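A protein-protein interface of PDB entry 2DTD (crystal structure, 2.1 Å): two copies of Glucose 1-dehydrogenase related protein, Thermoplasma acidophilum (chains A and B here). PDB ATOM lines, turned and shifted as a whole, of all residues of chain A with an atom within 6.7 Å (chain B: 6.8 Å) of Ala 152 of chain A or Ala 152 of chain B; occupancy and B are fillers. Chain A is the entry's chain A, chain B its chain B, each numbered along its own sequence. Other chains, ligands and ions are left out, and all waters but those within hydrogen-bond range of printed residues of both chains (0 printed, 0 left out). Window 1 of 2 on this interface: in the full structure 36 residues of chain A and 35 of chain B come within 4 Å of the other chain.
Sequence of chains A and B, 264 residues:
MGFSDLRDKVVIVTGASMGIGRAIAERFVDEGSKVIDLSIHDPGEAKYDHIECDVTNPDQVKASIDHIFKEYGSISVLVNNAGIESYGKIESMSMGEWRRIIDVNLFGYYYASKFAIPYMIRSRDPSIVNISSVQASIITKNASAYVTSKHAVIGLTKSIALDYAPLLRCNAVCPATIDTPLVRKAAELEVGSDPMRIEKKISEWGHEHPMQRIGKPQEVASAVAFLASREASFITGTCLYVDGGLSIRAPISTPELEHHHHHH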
ATOM      1  N   ILE A 102     -18.856  -4.750   9.067  1.00  0.00           N
ATOM      2  CA  ILE A 102     -18.824  -4.074  10.361  1.00  0.00           C
ATOM      3  C   ILE A 102     -20.087  -3.206  10.550  1.00  0.00           C
ATOM      4  O   ILE A 102     -20.636  -3.108  11.660  1.00  0.00           O
ATOM      5  CB  ILE A 102     -17.585  -3.157  10.474  1.00  0.00           C
ATOM      6  CG1 ILE A 102     -16.303  -3.967  10.229  1.00  0.00           C
ATOM      7  CG2 ILE A 102     -17.549  -2.479  11.838  1.00  0.00           C
ATOM      8  CD1 ILE A 102     -16.171  -5.230  11.081  1.00  0.00           C
ATOM      9  N   LEU A 106     -22.028  -4.693  13.582  1.00  0.00           N
ATOM     10  CA  LEU A 106     -21.776  -3.897  14.772  1.00  0.00           C
ATOM     11  C   LEU A 106     -22.611  -2.609  14.848  1.00  0.00           C
ATOM     12  O   LEU A 106     -23.335  -2.395  15.820  1.00  0.00           O
ATOM     13  CB  LEU A 106     -20.288  -3.544  14.881  1.00  0.00           C
ATOM     14  CG  LEU A 106     -19.966  -2.492  15.948  1.00  0.00           C
ATOM     15  CD1 LEU A 106     -20.294  -3.029  17.338  1.00  0.00           C
ATOM     16  CD2 LEU A 106     -18.505  -2.091  15.846  1.00  0.00           C
ATOM     17  N   SER A 132     -24.082 -12.732  19.272  1.00  0.00           N
ATOM     18  CA  SER A 132     -22.697 -12.630  18.866  1.00  0.00           C
ATOM     19  C   SER A 132     -22.373 -13.932  18.129  1.00  0.00           C
ATOM     20  O   SER A 132     -23.059 -14.290  17.175  1.00  0.00           O
ATOM     21  CB  SER A 132     -21.796 -12.451  20.096  1.00  0.00           C
ATOM     22  OG  SER A 132     -20.439 -12.306  19.727  1.00  0.00           O
ATOM     23  N   VAL A 147     -15.303 -11.955  12.208  1.00  0.00           N
ATOM     24  CA  VAL A 147     -14.712 -12.220  13.516  1.00  0.00           C
ATOM     25  C   VAL A 147     -14.525 -10.916  14.283  1.00  0.00           C
ATOM     26  O   VAL A 147     -14.819 -10.834  15.480  1.00  0.00           O
ATOM     27  CB  VAL A 147     -13.340 -12.946  13.365  1.00  0.00           C
ATOM     28  CG1 VAL A 147     -12.624 -13.022  14.701  1.00  0.00           C
ATOM     29  CG2 VAL A 147     -13.566 -14.352  12.824  1.00  0.00           C
ATOM     30  N   THR A 148     -14.038  -9.894  13.592  1.00  0.00           N
ATOM     31  CA  THR A 148     -13.834  -8.605  14.233  1.00  0.00           C
ATOM     32  C   THR A 148     -15.164  -8.056  14.737  1.00  0.00           C
ATOM     33  O   THR A 148     -15.267  -7.616  15.882  1.00  0.00           O
ATOM     34  CB  THR A 148     -13.193  -7.600  13.264  1.00  0.00           C
ATOM     35  OG1 THR A 148     -11.901  -8.087  12.877  1.00  0.00           O
ATOM     36  CG2 THR A 148     -13.020  -6.237  13.930  1.00  0.00           C
ATOM     37  N   SER A 149     -16.189  -8.113  13.896  1.00  0.00           N
ATOM     38  CA  SER A 149     -17.494  -7.600  14.284  1.00  0.00           C
ATOM     39  C   SER A 149     -18.065  -8.350  15.493  1.00  0.00           C
ATOM     40  O   SER A 149     -18.623  -7.726  16.391  1.00  0.00           O
ATOM     41  CB  SER A 149     -18.482  -7.659  13.103  1.00  0.00           C
ATOM     42  OG  SER A 149     -18.879  -8.990  12.780  1.00  0.00           O
ATOM     43  N   LYS A 150     -17.924  -9.672  15.529  1.00  0.00           N
ATOM     44  CA  LYS A 150     -18.455 -10.439  16.656  1.00  0.00           C
ATOM     45  C   LYS A 150     -17.737 -10.157  17.987  1.00  0.00           C
ATOM     46  O   LYS A 150     -18.355 -10.224  19.051  1.00  0.00           O
ATOM     47  CB  LYS A 150     -18.450 -11.938  16.334  1.00  0.00           C
ATOM     48  CG  LYS A 150     -19.427 -12.314  15.233  1.00  0.00           C
ATOM     49  CD  LYS A 150     -20.825 -11.810  15.576  1.00  0.00           C
ATOM     50  CE  LYS A 150     -21.843 -12.126  14.481  1.00  0.00           C
ATOM     51  NZ  LYS A 150     -23.254 -12.039  15.008  1.00  0.00           N
ATOM     52  N   HIS A 151     -16.441  -9.854  17.938  1.00  0.00           N
ATOM     53  CA  HIS A 151     -15.702  -9.508  19.155  1.00  0.00           C
ATOM     54  C   HIS A 151     -16.227  -8.132  19.593  1.00  0.00           C
ATOM     55  O   HIS A 151     -16.482  -7.893  20.778  1.00  0.00           O
ATOM     56  CB  HIS A 151     -14.189  -9.403  18.885  1.00  0.00           C
ATOM     57  CG  HIS A 151     -13.466 -10.716  18.935  1.00  0.00           C
ATOM     58  ND1 HIS A 151     -13.635 -11.700  17.985  1.00  0.00           N
ATOM     59  CD2 HIS A 151     -12.577 -11.208  19.832  1.00  0.00           C
ATOM     60  CE1 HIS A 151     -12.881 -12.741  18.293  1.00  0.00           C
ATOM     61  NE2 HIS A 151     -12.229 -12.469  19.409  1.00  0.00           N
ATOM     62  N   ALA A 152     -16.384  -7.231  18.624  1.00  0.00           N
ATOM     63  CA  ALA A 152     -16.879  -5.882  18.909  1.00  0.00           C
ATOM     64  C   ALA A 152     -18.239  -5.936  19.600  1.00  0.00           C
ATOM     65  O   ALA A 152     -18.488  -5.180  20.549  1.00  0.00           O
ATOM     66  CB  ALA A 152     -16.965  -5.064  17.620  1.00  0.00           C
ATOM     67  N   VAL A 153     -19.117  -6.830  19.141  1.00  0.00           N
ATOM     68  CA  VAL A 153     -20.445  -6.971  19.752  1.00  0.00           C
ATOM     69  C   VAL A 153     -20.342  -7.304  21.248  1.00  0.00           C
ATOM     70  O   VAL A 153     -21.161  -6.856  22.052  1.00  0.00           O
ATOM     71  CB  VAL A 153     -21.285  -8.069  19.034  1.00  0.00           C
ATOM     72  CG1 VAL A 153     -22.527  -8.406  19.852  1.00  0.00           C
ATOM     73  CG2 VAL A 153     -21.693  -7.561  17.634  1.00  0.00           C
ATOM     74  N   ILE A 154     -19.354  -8.108  21.621  1.00  0.00           N
ATOM     75  CA  ILE A 154     -19.166  -8.433  23.031  1.00  0.00           C
ATOM     76  C   ILE A 154     -18.814  -7.143  23.793  1.00  0.00           C
ATOM     77  O   ILE A 154     -19.294  -6.910  24.903  1.00  0.00           O
ATOM     78  CB  ILE A 154     -18.025  -9.468  23.227  1.00  0.00           C
ATOM     79  CG1 ILE A 154     -18.394 -10.785  22.541  1.00  0.00           C
ATOM     80  CG2 ILE A 154     -17.776  -9.696  24.721  1.00  0.00           C
ATOM     81  CD1 ILE A 154     -19.727 -11.347  22.992  1.00  0.00           C
ATOM     82  N   GLY A 155     -17.982  -6.296  23.190  1.00  0.00           N
ATOM     83  CA  GLY A 155     -17.610  -5.055  23.857  1.00  0.00           C
ATOM     84  C   GLY A 155     -18.804  -4.133  24.044  1.00  0.00           C
ATOM     85  O   GLY A 155     -18.996  -3.535  25.113  1.00  0.00           O
ATOM     86  N   LEU A 156     -19.612  -4.011  22.997  1.00  0.00           N
ATOM     87  CA  LEU A 156     -20.810  -3.172  23.047  1.00  0.00           C
ATOM     88  C   LEU A 156     -21.755  -3.695  24.137  1.00  0.00           C
ATOM     89  O   LEU A 156     -22.353  -2.917  24.890  1.00  0.00           O
ATOM     90  CB  LEU A 156     -21.525  -3.181  21.683  1.00  0.00           C
ATOM     91  CG  LEU A 156     -22.835  -2.378  21.598  1.00  0.00           C
ATOM     92  CD1 LEU A 156     -22.547  -0.893  21.772  1.00  0.00           C
ATOM     93  CD2 LEU A 156     -23.522  -2.625  20.271  1.00  0.00           C
ATOM     94  N   THR A 157     -21.877  -5.016  24.216  1.00  0.00           N
ATOM     95  CA  THR A 157     -22.740  -5.667  25.203  1.00  0.00           C
ATOM     96  C   THR A 157     -22.340  -5.353  26.649  1.00  0.00           C
ATOM     97  O   THR A 157     -23.198  -5.026  27.477  1.00  0.00           O
ATOM     98  CB  THR A 157     -22.735  -7.187  24.997  1.00  0.00           C
ATOM     99  OG1 THR A 157     -23.244  -7.475  23.692  1.00  0.00           O
ATOM    100  CG2 THR A 157     -23.613  -7.895  26.064  1.00  0.00           C
ATOM    101  N   ILE B 102     -14.259   4.450  16.514  1.00  0.00           N
ATOM    102  CA  ILE B 102     -14.116   3.141  15.873  1.00  0.00           C
ATOM    103  C   ILE B 102     -13.152   3.229  14.679  1.00  0.00           C
ATOM    104  O   ILE B 102     -12.348   2.315  14.436  1.00  0.00           O
ATOM    105  CB  ILE B 102     -15.479   2.607  15.361  1.00  0.00           C
ATOM    106  CG1 ILE B 102     -16.497   2.538  16.516  1.00  0.00           C
ATOM    107  CG2 ILE B 102     -15.297   1.227  14.734  1.00  0.00           C
ATOM    108  CD1 ILE B 102     -16.055   1.700  17.714  1.00  0.00           C
ATOM    109  N   ASN B 105      -9.411   3.724  16.314  1.00  0.00           N
ATOM    110  CA  ASN B 105      -9.003   2.576  17.117  1.00  0.00           C
ATOM    111  C   ASN B 105      -9.098   1.223  16.421  1.00  0.00           C
ATOM    112  O   ASN B 105      -8.409   0.274  16.806  1.00  0.00           O
ATOM    113  CB  ASN B 105      -9.806   2.552  18.428  1.00  0.00           C
ATOM    114  CG  ASN B 105      -9.503   3.749  19.318  1.00  0.00           C
ATOM    115  OD1 ASN B 105      -8.800   4.669  18.904  1.00  0.00           O
ATOM    116  ND2 ASN B 105     -10.036   3.746  20.539  1.00  0.00           N
ATOM    117  N   LEU B 106      -9.943   1.125  15.404  1.00  0.00           N
ATOM    118  CA  LEU B 106     -10.089  -0.134  14.693  1.00  0.00           C
ATOM    119  C   LEU B 106      -9.667  -0.051  13.238  1.00  0.00           C
ATOM    120  O   LEU B 106      -8.714  -0.709  12.833  1.00  0.00           O
ATOM    121  CB  LEU B 106     -11.535  -0.639  14.757  1.00  0.00           C
ATOM    122  CG  LEU B 106     -11.777  -1.856  13.863  1.00  0.00           C
ATOM    123  CD1 LEU B 106     -10.905  -3.032  14.351  1.00  0.00           C
ATOM    124  CD2 LEU B 106     -13.252  -2.217  13.878  1.00  0.00           C
ATOM    125  N   SER B 132      -4.124  -3.077  22.436  1.00  0.00           N
ATOM    126  CA  SER B 132      -5.541  -3.115  22.768  1.00  0.00           C
ATOM    127  C   SER B 132      -5.684  -2.452  24.125  1.00  0.00           C
ATOM    128  O   SER B 132      -5.268  -1.311  24.302  1.00  0.00           O
ATOM    129  CB  SER B 132      -6.043  -4.559  22.833  1.00  0.00           C
ATOM    130  OG  SER B 132      -7.428  -4.598  23.117  1.00  0.00           O
ATOM    131  N   ALA B 136     -10.418  -4.933  27.079  1.00  0.00           N
ATOM    132  CA  ALA B 136     -10.857  -5.917  26.108  1.00  0.00           C
ATOM    133  C   ALA B 136     -11.432  -7.032  26.999  1.00  0.00           C
ATOM    134  O   ALA B 136     -11.966  -8.028  26.525  1.00  0.00           O
ATOM    135  CB  ALA B 136      -9.673  -6.433  25.307  1.00  0.00           C
ATOM    136  N   VAL B 147     -14.449   0.959  24.432  1.00  0.00           N
ATOM    137  CA  VAL B 147     -14.489  -0.449  24.838  1.00  0.00           C
ATOM    138  C   VAL B 147     -14.770  -1.380  23.665  1.00  0.00           C
ATOM    139  O   VAL B 147     -14.166  -2.453  23.546  1.00  0.00           O
ATOM    140  CB  VAL B 147     -15.566  -0.680  25.943  1.00  0.00           C
ATOM    141  CG1 VAL B 147     -15.772  -2.177  26.193  1.00  0.00           C
ATOM    142  CG2 VAL B 147     -15.137   0.018  27.227  1.00  0.00           C
ATOM    143  N   THR B 148     -15.696  -0.969  22.807  1.00  0.00           N
ATOM    144  CA  THR B 148     -16.046  -1.763  21.637  1.00  0.00           C
ATOM    145  C   THR B 148     -14.842  -1.866  20.695  1.00  0.00           C
ATOM    146  O   THR B 148     -14.518  -2.950  20.204  1.00  0.00           O
ATOM    147  CB  THR B 148     -17.221  -1.135  20.860  1.00  0.00           C
ATOM    148  OG1 THR B 148     -18.404  -1.144  21.675  1.00  0.00           O
ATOM    149  CG2 THR B 148     -17.479  -1.917  19.584  1.00  0.00           C
ATOM    150  N   SER B 149     -14.177  -0.740  20.447  1.00  0.00           N
ATOM    151  CA  SER B 149     -13.029  -0.764  19.556  1.00  0.00           C
ATOM    152  C   SER B 149     -11.907  -1.660  20.088  1.00  0.00           C
ATOM    153  O   SER B 149     -11.228  -2.319  19.313  1.00  0.00           O
ATOM    154  CB  SER B 149     -12.505   0.660  19.290  1.00  0.00           C
ATOM    155  OG  SER B 149     -11.934   1.267  20.441  1.00  0.00           O
ATOM    156  N   LYS B 150     -11.728  -1.701  21.406  1.00  0.00           N
ATOM    157  CA  LYS B 150     -10.672  -2.511  21.994  1.00  0.00           C
ATOM    158  C   LYS B 150     -10.984  -4.002  21.915  1.00  0.00           C
ATOM    159  O   LYS B 150     -10.070  -4.822  21.829  1.00  0.00           O
ATOM    160  CB  LYS B 150     -10.401  -2.066  23.437  1.00  0.00           C
ATOM    161  CG  LYS B 150      -9.734  -0.680  23.524  1.00  0.00           C
ATOM    162  CD  LYS B 150      -8.486  -0.612  22.630  1.00  0.00           C
ATOM    163  CE  LYS B 150      -7.809   0.761  22.656  1.00  0.00           C
ATOM    164  NZ  LYS B 150      -6.565   0.782  21.806  1.00  0.00           N
ATOM    165  N   HIS B 151     -12.270  -4.357  21.945  1.00  0.00           N
ATOM    166  CA  HIS B 151     -12.673  -5.758  21.809  1.00  0.00           C
ATOM    167  C   HIS B 151     -12.467  -6.129  20.330  1.00  0.00           C
ATOM    168  O   HIS B 151     -11.983  -7.225  19.998  1.00  0.00           O
ATOM    169  CB  HIS B 151     -14.150  -5.951  22.178  1.00  0.00           C
ATOM    170  CG  HIS B 151     -14.403  -6.113  23.647  1.00  0.00           C
ATOM    171  ND1 HIS B 151     -14.227  -5.091  24.557  1.00  0.00           N
ATOM    172  CD2 HIS B 151     -14.842  -7.179  24.360  1.00  0.00           C
ATOM    173  CE1 HIS B 151     -14.550  -5.519  25.767  1.00  0.00           C
ATOM    174  NE2 HIS B 151     -14.929  -6.782  25.674  1.00  0.00           N
ATOM    175  N   ALA B 152     -12.830  -5.204  19.443  1.00  0.00           N
ATOM    176  CA  ALA B 152     -12.688  -5.424  18.005  1.00  0.00           C
ATOM    177  C   ALA B 152     -11.222  -5.665  17.646  1.00  0.00           C
ATOM    178  O   ALA B 152     -10.908  -6.507  16.803  1.00  0.00           O
ATOM    179  CB  ALA B 152     -13.244  -4.212  17.211  1.00  0.00           C
ATOM    180  N   VAL B 153     -10.324  -4.915  18.271  1.00  0.00           N
ATOM    181  CA  VAL B 153      -8.903  -5.104  17.997  1.00  0.00           C
ATOM    182  C   VAL B 153      -8.489  -6.547  18.309  1.00  0.00           C
ATOM    183  O   VAL B 153      -7.680  -7.139  17.593  1.00  0.00           O
ATOM    184  CB  VAL B 153      -8.053  -4.111  18.812  1.00  0.00           C
ATOM    185  CG1 VAL B 153      -6.558  -4.511  18.762  1.00  0.00           C
ATOM    186  CG2 VAL B 153      -8.229  -2.704  18.220  1.00  0.00           C
ATOM    187  N   ILE B 154      -9.047  -7.122  19.372  1.00  0.00           N
ATOM    188  CA  ILE B 154      -8.721  -8.504  19.711  1.00  0.00           C
ATOM    189  C   ILE B 154      -9.149  -9.440  18.578  1.00  0.00           C
ATOM    190  O   ILE B 154      -8.419 -10.366  18.215  1.00  0.00           O
ATOM    191  CB  ILE B 154      -9.415  -8.954  21.007  1.00  0.00           C
ATOM    192  CG1 ILE B 154      -8.951  -8.078  22.176  1.00  0.00           C
ATOM    193  CG2 ILE B 154      -9.114 -10.434  21.263  1.00  0.00           C
ATOM    194  CD1 ILE B 154      -7.456  -8.047  22.371  1.00  0.00           C
ATOM    195  N   GLY B 155     -10.336  -9.206  18.027  1.00  0.00           N
ATOM    196  CA  GLY B 155     -10.819 -10.039  16.938  1.00  0.00           C
ATOM    197  C   GLY B 155      -9.953  -9.922  15.687  1.00  0.00           C
ATOM    198  O   GLY B 155      -9.693 -10.910  15.004  1.00  0.00           O
ATOM    199  N   LEU B 156      -9.506  -8.709  15.380  1.00  0.00           N
ATOM    200  CA  LEU B 156      -8.673  -8.486  14.205  1.00  0.00           C
ATOM    201  C   LEU B 156      -7.323  -9.193  14.377  1.00  0.00           C
ATOM    202  O   LEU B 156      -6.781  -9.753  13.433  1.00  0.00           O
ATOM    203  CB  LEU B 156      -8.444  -6.992  13.994  1.00  0.00           C
ATOM    204  CG  LEU B 156      -7.581  -6.622  12.781  1.00  0.00           C
ATOM    205  CD1 LEU B 156      -8.309  -6.972  11.477  1.00  0.00           C
ATOM    206  CD2 LEU B 156      -7.275  -5.131  12.841  1.00  0.00           C
ATOM    207  N   THR B 157      -6.798  -9.141  15.594  1.00  0.00           N
ATOM    208  CA  THR B 157      -5.528  -9.765  15.940  1.00  0.00           C
ATOM    209  C   THR B 157      -5.592 -11.279  15.722  1.00  0.00           C
ATOM    210  O   THR B 157      -4.709 -11.861  15.098  1.00  0.00           O
ATOM    211  CB  THR B 157      -5.183  -9.504  17.418  1.00  0.00           C
ATOM    212  OG1 THR B 157      -4.974  -8.105  17.620  1.00  0.00           O
ATOM    213  CG2 THR B 157      -3.932 -10.265  17.829  1.00  0.00           C
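Ala 152 of chain A touches two residues of chain B.
Ala 152 of chain B touches just these residues of chain A: Thr 148 (3.6 Å) and Ala 152 (3.8 Å).
Printed residues of chain B within 4 Å of His 151 of chain A: His 151, Ile 154 and Gly 155.
Of the printed residues of chain B, Gly 155 of chain A touches Val 147 (3.7 Å), Thr 148 (3.8 Å) and His 151 (3.4 Å).
The nearest residue of chain A that does not touch Ala 152 of chain B is His 151 of chain A (4.3 Å).
The nearest printed residue of chain A that does not touch His 151 of chain B is Ala 152 of chain A (4.3 Å).
O of Val 147 of chain A sits at hydrogen-bond distance from ND1 of His 151 of chain A (2.9 Å).
A ring nitrogen (ND1) of His 151 of chain B sits at hydrogen-bond distance from the backbone carbonyl oxygen (O) of Val 147 of chain B, at 2.8 Å.
A ring nitrogen (NE2) of His 151 of chain B is in hydrogen-bond range of the backbone carbonyl oxygen of Ala 136 of chain B (3.3 Å).
Leu 106 of chain A touches Thr 148 of chain B, and with the chains exchanged Thr 148 of chain A touches Leu 106 of chain B.
Thr 148 of chain A touches Ala 152 of chain B, and with the chains exchanged Ala 152 of chain A touches Thr 148 of chain B.
Thr 148 of chain A touches Gly 155 of chain B, and with the chains exchanged Gly 155 of chain A touches Thr 148 of chain B.
Thr 148 of chain A touches Leu 156 of chain B, and with the chains exchanged Leu 156 of chain A touches Thr 148 of chain B.
14 positions are printed for both chains.
Of the 16 pairs that touch across the chains among the printed residues, 16 have their exchanged pair printed and touching as well.
Printed residues of chain A that touch a printed residue of chain B: Leu 106, Val 147, Thr 148, His 151, Ala 152, Ile 154, Gly 155 and Leu 156.
Along chain A the printed residues that touch a printed residue of chain B span positions 106 to 156.
Among the printed residues, no Asp or Glu carboxylate lies within 4 Å of a Lys or Arg side-chain nitrogen of the other chain.
Gly 155 of chain B touches Val 147 of chain A (O to CG1, 3.6 Å).
Thr 148 of chain A touches Leu 106 of chain B (CG2 to CD1, 3.9 Å).
CG2 of Thr 148 of chain A touches O of Ala 152 of chain B, at 3.6 Å.
Gly 155 of chain B touches Thr 148 of chain A (C to OG1, 3.9 Å).
Leu 156 of chain B touches Thr 148 of chain A.
His 151 of chain B touches His 151 of chain A (O to CB, 3.3 Å).
His 151 of chain A touches Ile 154 of chain B (CD2 to CG2, 3.8 Å).
CG of His 151 of chain A touches CA of Gly 155 of chain B, at 3.4 Å.
Val 147 of chain B touches Gly 155 of chain A.
His 151 of chain B touches Gly 155 of chain A (CG to CA, 3.4 Å).
OG1 of Thr 148 of chain B sits at hydrogen-bond distance from N of Leu 156 of chain A, at 3.4 Å.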
